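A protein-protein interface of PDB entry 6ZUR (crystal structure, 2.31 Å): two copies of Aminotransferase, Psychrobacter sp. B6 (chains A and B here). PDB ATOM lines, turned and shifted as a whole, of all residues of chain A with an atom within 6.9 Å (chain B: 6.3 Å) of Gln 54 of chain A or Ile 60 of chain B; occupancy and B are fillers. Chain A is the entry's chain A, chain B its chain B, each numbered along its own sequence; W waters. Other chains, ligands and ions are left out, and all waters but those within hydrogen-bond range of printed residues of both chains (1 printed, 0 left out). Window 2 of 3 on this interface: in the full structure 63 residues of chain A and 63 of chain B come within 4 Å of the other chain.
The backbone carbonyl oxygen of Ser 61 of chain B lies within hydrogen-bond range of the guanidinium group of Arg 63 of chain B, at 2.9 Å.
The side-chain hydroxyl (OG) of Ser 61 of chain B is in hydrogen-bond range of the backbone carbonyl oxygen (O) of Pro 59 of chain B (3.2 Å).
Val 45 of chain A touches Ile 60 of chain B.
CG2 of Val 45 of chain A touches O of Ser 61 of chain B, at 3.5 Å.
Pro 62 of chain B touches Val 45 of chain A.
CD1 of Ile 60 of chain B touches O of Lys 50 of chain A, 3.6 Å away.
CG2 of Ile 60 of chain B touches OE1 of Glu 53 of chain A, 3.2 Å away.
Gln 54 of chain A touches Ile 60 of chain B (CG to CD1, 3.96 Å).
Gln 54 of chain A touches just one residue of chain B: Ile 60.
Of the printed residues of chain A, Pro 62 of chain B touches Val 45.
Of the printed residues of chain B, Glu 53 of chain A touches Ile 60 (3.2 Å) and Arg 63 (2.6 Å).
Of the printed residues of chain A, Arg 63 of chain B touches Glu 53.
Of the printed residues of chain A, Ser 61 of chain B touches Val 45.
Leu 46 of chain A touches none of the printed residues of chain B.
The nearest residue of chain A that does not touch Ile 60 of chain B is Val 49 of chain A (5.4 Å).
The guanidinium group of Arg 63 of chain B lies within salt-bridge range of the side-chain carboxylate of Glu 53 of chain A (2.6 Å).
Hydrophobic or aromatic side chains of chain A within 4 Å of the printed part of chain B: Val 45.
Hydrophobic or aromatic side chains of chain B within 4 Å of the printed part of chain A: Ile 60.
Water W1 bridges OE2 of Glu 53 of chain A and NH1 of Arg 63 of chain B.
Positions printed for both chains: 56, 57, 58 and 59.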
ATOM      1  N   VAL A  45      30.024   4.438  16.775  1.00  0.00           N
ATOM      2  CA  VAL A  45      28.701   3.880  16.848  1.00  0.00           C
ATOM      3  C   VAL A  45      28.164   4.057  15.446  1.00  0.00           C
ATOM      4  O   VAL A  45      28.019   5.173  14.982  1.00  0.00           O
ATOM      5  CB  VAL A  45      27.823   4.666  17.814  1.00  0.00           C
ATOM      6  CG1 VAL A  45      26.405   4.140  17.824  1.00  0.00           C
ATOM      7  CG2 VAL A  45      28.371   4.593  19.216  1.00  0.00           C
ATOM      8  N   LEU A  46      27.819   2.954  14.785  1.00  0.00           N
ATOM      9  CA  LEU A  46      27.356   2.990  13.439  1.00  0.00           C
ATOM     10  C   LEU A  46      25.899   3.516  13.388  1.00  0.00           C
ATOM     11  O   LEU A  46      25.101   3.271  14.285  1.00  0.00           O
ATOM     12  CB  LEU A  46      27.449   1.641  12.793  1.00  0.00           C
ATOM     13  CG  LEU A  46      28.805   0.942  12.842  1.00  0.00           C
ATOM     14  CD1 LEU A  46      28.764  -0.361  12.047  1.00  0.00           C
ATOM     15  CD2 LEU A  46      29.852   1.876  12.296  1.00  0.00           C
ATOM     16  N   ASP A  47      25.599   4.283  12.336  1.00  0.00           N
ATOM     17  CA  ASP A  47      24.279   4.837  12.139  1.00  0.00           C
ATOM     18  C   ASP A  47      23.245   3.743  12.092  1.00  0.00           C
ATOM     19  O   ASP A  47      22.189   3.890  12.687  1.00  0.00           O
ATOM     20  CB  ASP A  47      24.231   5.674  10.863  1.00  0.00           C
ATOM     21  CG  ASP A  47      24.803   7.079  11.053  1.00  0.00           C
ATOM     22  OD1 ASP A  47      25.799   7.239  11.819  1.00  0.00           O
ATOM     23  OD2 ASP A  47      24.236   8.023  10.446  1.00  0.00           O
ATOM     24  N   VAL A  49      23.277   0.684  13.274  1.00  0.00           N
ATOM     25  CA  VAL A  49      23.132   0.194  14.635  1.00  0.00           C
ATOM     26  C   VAL A  49      22.325   1.116  15.522  1.00  0.00           C
ATOM     27  O   VAL A  49      21.406   0.669  16.234  1.00  0.00           O
ATOM     28  CB  VAL A  49      24.539  -0.093  15.265  1.00  0.00           C
ATOM     29  CG1 VAL A  49      24.485  -0.338  16.772  1.00  0.00           C
ATOM     30  CG2 VAL A  49      25.148  -1.307  14.580  1.00  0.00           C
ATOM     31  N   LYS A  50      22.695   2.388  15.539  1.00  0.00           N
ATOM     32  CA  LYS A  50      21.962   3.347  16.337  1.00  0.00           C
ATOM     33  C   LYS A  50      20.471   3.225  16.007  1.00  0.00           C
ATOM     34  O   LYS A  50      19.643   3.116  16.893  1.00  0.00           O
ATOM     35  CB  LYS A  50      22.510   4.735  16.029  1.00  0.00           C
ATOM     36  CG  LYS A  50      21.939   5.792  16.895  1.00  0.00           C
ATOM     37  CD  LYS A  50      22.650   7.109  16.734  1.00  0.00           C
ATOM     38  CE  LYS A  50      22.252   8.034  17.896  1.00  0.00           C
ATOM     39  NZ  LYS A  50      22.370   9.506  17.635  1.00  0.00           N
ATOM     40  N   ILE A  51      20.140   3.133  14.730  1.00  0.00           N
ATOM     41  CA  ILE A  51      18.766   3.008  14.346  1.00  0.00           C
ATOM     42  C   ILE A  51      18.167   1.686  14.844  1.00  0.00           C
ATOM     43  O   ILE A  51      17.020   1.628  15.318  1.00  0.00           O
ATOM     44  CB  ILE A  51      18.585   3.159  12.822  1.00  0.00           C
ATOM     45  CG1 ILE A  51      18.935   4.581  12.366  1.00  0.00           C
ATOM     46  CG2 ILE A  51      17.138   2.902  12.415  1.00  0.00           C
ATOM     47  CD1 ILE A  51      19.118   4.684  10.828  1.00  0.00           C
ATOM     48  N   ALA A  52      18.929   0.629  14.738  1.00  0.00           N
ATOM     49  CA  ALA A  52      18.452  -0.662  15.194  1.00  0.00           C
ATOM     50  C   ALA A  52      18.133  -0.608  16.689  1.00  0.00           C
ATOM     51  O   ALA A  52      17.131  -1.155  17.133  1.00  0.00           O
ATOM     52  CB  ALA A  52      19.472  -1.739  14.892  1.00  0.00           C
ATOM     53  N   GLU A  53      18.953   0.086  17.436  1.00  0.00           N
ATOM     54  CA  GLU A  53      18.783   0.136  18.879  1.00  0.00           C
ATOM     55  C   GLU A  53      17.600   1.008  19.329  1.00  0.00           C
ATOM     56  O   GLU A  53      16.865   0.605  20.217  1.00  0.00           O
ATOM     57  CB  GLU A  53      20.085   0.502  19.579  1.00  0.00           C
ATOM     58  CG  GLU A  53      21.131  -0.581  19.409  1.00  0.00           C
ATOM     59  CD  GLU A  53      22.388  -0.360  20.281  1.00  0.00           C
ATOM     60  OE1 GLU A  53      23.060   0.670  20.172  1.00  0.00           O
ATOM     61  OE2 GLU A  53      22.726  -1.247  21.019  1.00  0.00           O
ATOM     62  N   GLN A  54      17.368   2.119  18.643  1.00  0.00           N
ATOM     63  CA  GLN A  54      16.151   2.882  18.855  1.00  0.00           C
ATOM     64  C   GLN A  54      14.894   2.059  18.602  1.00  0.00           C
ATOM     65  O   GLN A  54      13.886   2.201  19.338  1.00  0.00           O
ATOM     66  CB  GLN A  54      16.163   4.125  17.992  1.00  0.00           C
ATOM     67  CG  GLN A  54      17.122   5.138  18.578  1.00  0.00           C
ATOM     68  CD  GLN A  54      17.644   6.182  17.625  1.00  0.00           C
ATOM     69  OE1 GLN A  54      17.474   6.099  16.394  1.00  0.00           O
ATOM     70  NE2 GLN A  54      18.349   7.179  18.198  1.00  0.00           N
ATOM     71  N   ARG A  55      14.950   1.156  17.641  1.00  0.00           N
ATOM     72  CA  ARG A  55      13.818   0.283  17.392  1.00  0.00           C
ATOM     73  C   ARG A  55      13.663  -0.699  18.551  1.00  0.00           C
ATOM     74  O   ARG A  55      12.550  -1.052  18.922  1.00  0.00           O
ATOM     75  CB  ARG A  55      13.973  -0.467  16.080  1.00  0.00           C
ATOM     76  CG  ARG A  55      13.817   0.404  14.836  1.00  0.00           C
ATOM     77  CD  ARG A  55      13.656  -0.430  13.564  1.00  0.00           C
ATOM     78  NE  ARG A  55      13.964   0.382  12.385  1.00  0.00           N
ATOM     79  CZ  ARG A  55      14.052  -0.094  11.134  1.00  0.00           C
ATOM     80  NH1 ARG A  55      13.835  -1.391  10.888  1.00  0.00           N
ATOM     81  NH2 ARG A  55      14.377   0.710  10.150  1.00  0.00           N
ATOM     82  N   ILE A  56      14.796  -1.143  19.112  1.00  0.00           N
ATOM     83  CA  ILE A  56      14.805  -2.133  20.196  1.00  0.00           C
ATOM     84  C   ILE A  56      14.295  -1.470  21.445  1.00  0.00           C
ATOM     85  O   ILE A  56      13.640  -2.124  22.273  1.00  0.00           O
ATOM     86  CB  ILE A  56      16.213  -2.750  20.413  1.00  0.00           C
ATOM     87  CG1 ILE A  56      16.553  -3.723  19.261  1.00  0.00           C
ATOM     88  CG2 ILE A  56      16.276  -3.455  21.750  1.00  0.00           C
ATOM     89  CD1 ILE A  56      18.022  -4.091  19.108  1.00  0.00           C
ATOM     90  N   ALA A  57      14.635  -0.196  21.633  1.00  0.00           N
ATOM     91  CA  ALA A  57      14.169   0.531  22.808  1.00  0.00           C
ATOM     92  C   ALA A  57      12.721   1.070  22.695  1.00  0.00           C
ATOM     93  O   ALA A  57      12.217   1.576  23.662  1.00  0.00           O
ATOM     94  CB  ALA A  57      15.127   1.664  23.136  1.00  0.00           C
ATOM     95  N   ASP A  58      12.068   0.900  21.542  1.00  0.00           N
ATOM     96  CA  ASP A  58      10.751   1.448  21.243  1.00  0.00           C
ATOM     97  C   ASP A  58       9.777   0.393  20.655  1.00  0.00           C
ATOM     98  O   ASP A  58       9.751   0.201  19.452  1.00  0.00           O
ATOM     99  CB  ASP A  58      10.841   2.591  20.240  1.00  0.00           C
ATOM    100  CG  ASP A  58       9.461   3.192  19.962  1.00  0.00           C
ATOM    101  OD1 ASP A  58       8.763   3.559  20.955  1.00  0.00           O
ATOM    102  OD2 ASP A  58       9.056   3.205  18.787  1.00  0.00           O
ATOM    103  N   PRO A  59       8.971  -0.282  21.483  1.00  0.00           N
ATOM    104  CA  PRO A  59       9.045  -0.146  22.933  1.00  0.00           C
ATOM    105  C   PRO A  59      10.041  -1.183  23.542  1.00  0.00           C
ATOM    106  O   PRO A  59      10.379  -2.190  22.913  1.00  0.00           O
ATOM    107  CB  PRO A  59       7.636  -0.510  23.352  1.00  0.00           C
ATOM    108  CG  PRO A  59       7.322  -1.669  22.423  1.00  0.00           C
ATOM    109  CD  PRO A  59       8.127  -1.450  21.140  1.00  0.00           C
ATOM    110  N   ILE B  56      20.448   3.411  29.319  1.00  0.00           N
ATOM    111  CA  ILE B  56      21.334   2.775  28.322  1.00  0.00           C
ATOM    112  C   ILE B  56      21.125   3.327  26.932  1.00  0.00           C
ATOM    113  O   ILE B  56      22.066   3.442  26.162  1.00  0.00           O
ATOM    114  CB  ILE B  56      21.175   1.214  28.314  1.00  0.00           C
ATOM    115  CG1 ILE B  56      21.684   0.672  29.643  1.00  0.00           C
ATOM    116  CG2 ILE B  56      22.007   0.612  27.171  1.00  0.00           C
ATOM    117  CD1 ILE B  56      21.426  -0.801  29.970  1.00  0.00           C
ATOM    118  N   ALA B  57      19.886   3.588  26.565  1.00  0.00           N
ATOM    119  CA  ALA B  57      19.619   4.171  25.254  1.00  0.00           C
ATOM    120  C   ALA B  57      19.801   5.714  25.140  1.00  0.00           C
ATOM    121  O   ALA B  57      19.608   6.269  24.059  1.00  0.00           O
ATOM    122  CB  ALA B  57      18.254   3.798  24.780  1.00  0.00           C
ATOM    123  N   ASP B  58      20.187   6.378  26.223  1.00  0.00           N
ATOM    124  CA  ASP B  58      20.236   7.849  26.306  1.00  0.00           C
ATOM    125  C   ASP B  58      21.560   8.281  26.887  1.00  0.00           C
ATOM    126  O   ASP B  58      21.643   8.446  28.081  1.00  0.00           O
ATOM    127  CB  ASP B  58      19.115   8.394  27.219  1.00  0.00           C
ATOM    128  CG  ASP B  58      19.240   9.907  27.462  1.00  0.00           C
ATOM    129  OD1 ASP B  58      18.930  10.690  26.538  1.00  0.00           O
ATOM    130  OD2 ASP B  58      19.666  10.287  28.570  1.00  0.00           O
ATOM    131  N   PRO B  59      22.604   8.427  26.070  1.00  0.00           N
ATOM    132  CA  PRO B  59      22.566   8.160  24.649  1.00  0.00           C
ATOM    133  C   PRO B  59      23.099   6.778  24.334  1.00  0.00           C
ATOM    134  O   PRO B  59      23.711   6.123  25.170  1.00  0.00           O
ATOM    135  CB  PRO B  59      23.552   9.181  24.116  1.00  0.00           C
ATOM    136  CG  PRO B  59      24.630   9.210  25.189  1.00  0.00           C
ATOM    137  CD  PRO B  59      23.960   8.852  26.486  1.00  0.00           C
ATOM    138  N   ILE B  60      22.915   6.387  23.095  1.00  0.00           N
ATOM    139  CA  ILE B  60      23.506   5.185  22.572  1.00  0.00           C
ATOM    140  C   ILE B  60      25.027   5.308  22.520  1.00  0.00           C
ATOM    141  O   ILE B  60      25.541   6.161  21.799  1.00  0.00           O
ATOM    142  CB  ILE B  60      22.937   4.874  21.207  1.00  0.00           C
ATOM    143  CG1 ILE B  60      21.482   4.365  21.408  1.00  0.00           C
ATOM    144  CG2 ILE B  60      23.769   3.774  20.556  1.00  0.00           C
ATOM    145  CD1 ILE B  60      20.685   4.387  20.135  1.00  0.00           C
ATOM    146  N   SER B  61      25.725   4.468  23.293  1.00  0.00           N
ATOM    147  CA  SER B  61      27.150   4.622  23.437  1.00  0.00           C
ATOM    148  C   SER B  61      28.016   3.655  22.586  1.00  0.00           C
ATOM    149  O   SER B  61      27.504   2.682  22.018  1.00  0.00           O
ATOM    150  CB  SER B  61      27.491   4.562  24.915  1.00  0.00           C
ATOM    151  OG  SER B  61      26.819   5.607  25.564  1.00  0.00           O
ATOM    152  N   PRO B  62      29.319   3.954  22.482  1.00  0.00           N
ATOM    153  CA  PRO B  62      30.259   3.025  21.826  1.00  0.00           C
ATOM    154  C   PRO B  62      30.235   1.704  22.569  1.00  0.00           C
ATOM    155  O   PRO B  62      29.854   1.678  23.736  1.00  0.00           O
ATOM    156  CB  PRO B  62      31.614   3.702  22.022  1.00  0.00           C
ATOM    157  CG  PRO B  62      31.309   5.144  22.214  1.00  0.00           C
ATOM    158  CD  PRO B  62      30.015   5.170  22.958  1.00  0.00           C
ATOM    159  N   ARG B  63      30.577   0.617  21.902  1.00  0.00           N
ATOM    160  CA  ARG B  63      30.359  -0.677  22.499  1.00  0.00           C
ATOM    161  C   ARG B  63      31.683  -1.474  22.575  1.00  0.00           C
ATOM    162  O   ARG B  63      31.841  -2.567  21.957  1.00  0.00           O
ATOM    163  CB  ARG B  63      29.244  -1.403  21.749  1.00  0.00           C
ATOM    164  CG  ARG B  63      28.315  -2.182  22.656  1.00  0.00           C
ATOM    165  CD  ARG B  63      27.512  -1.304  23.619  1.00  0.00           C
ATOM    166  NE  ARG B  63      26.933  -0.196  22.909  1.00  0.00           N
ATOM    167  CZ  ARG B  63      25.855  -0.273  22.075  1.00  0.00           C
ATOM    168  NH1 ARG B  63      25.204  -1.442  21.891  1.00  0.00           N
ATOM    169  NH2 ARG B  63      25.465   0.770  21.443  1.00  0.00           N
HETATM  170  O   HOH W   1      22.942   0.293  23.480  1.00  0.00           O
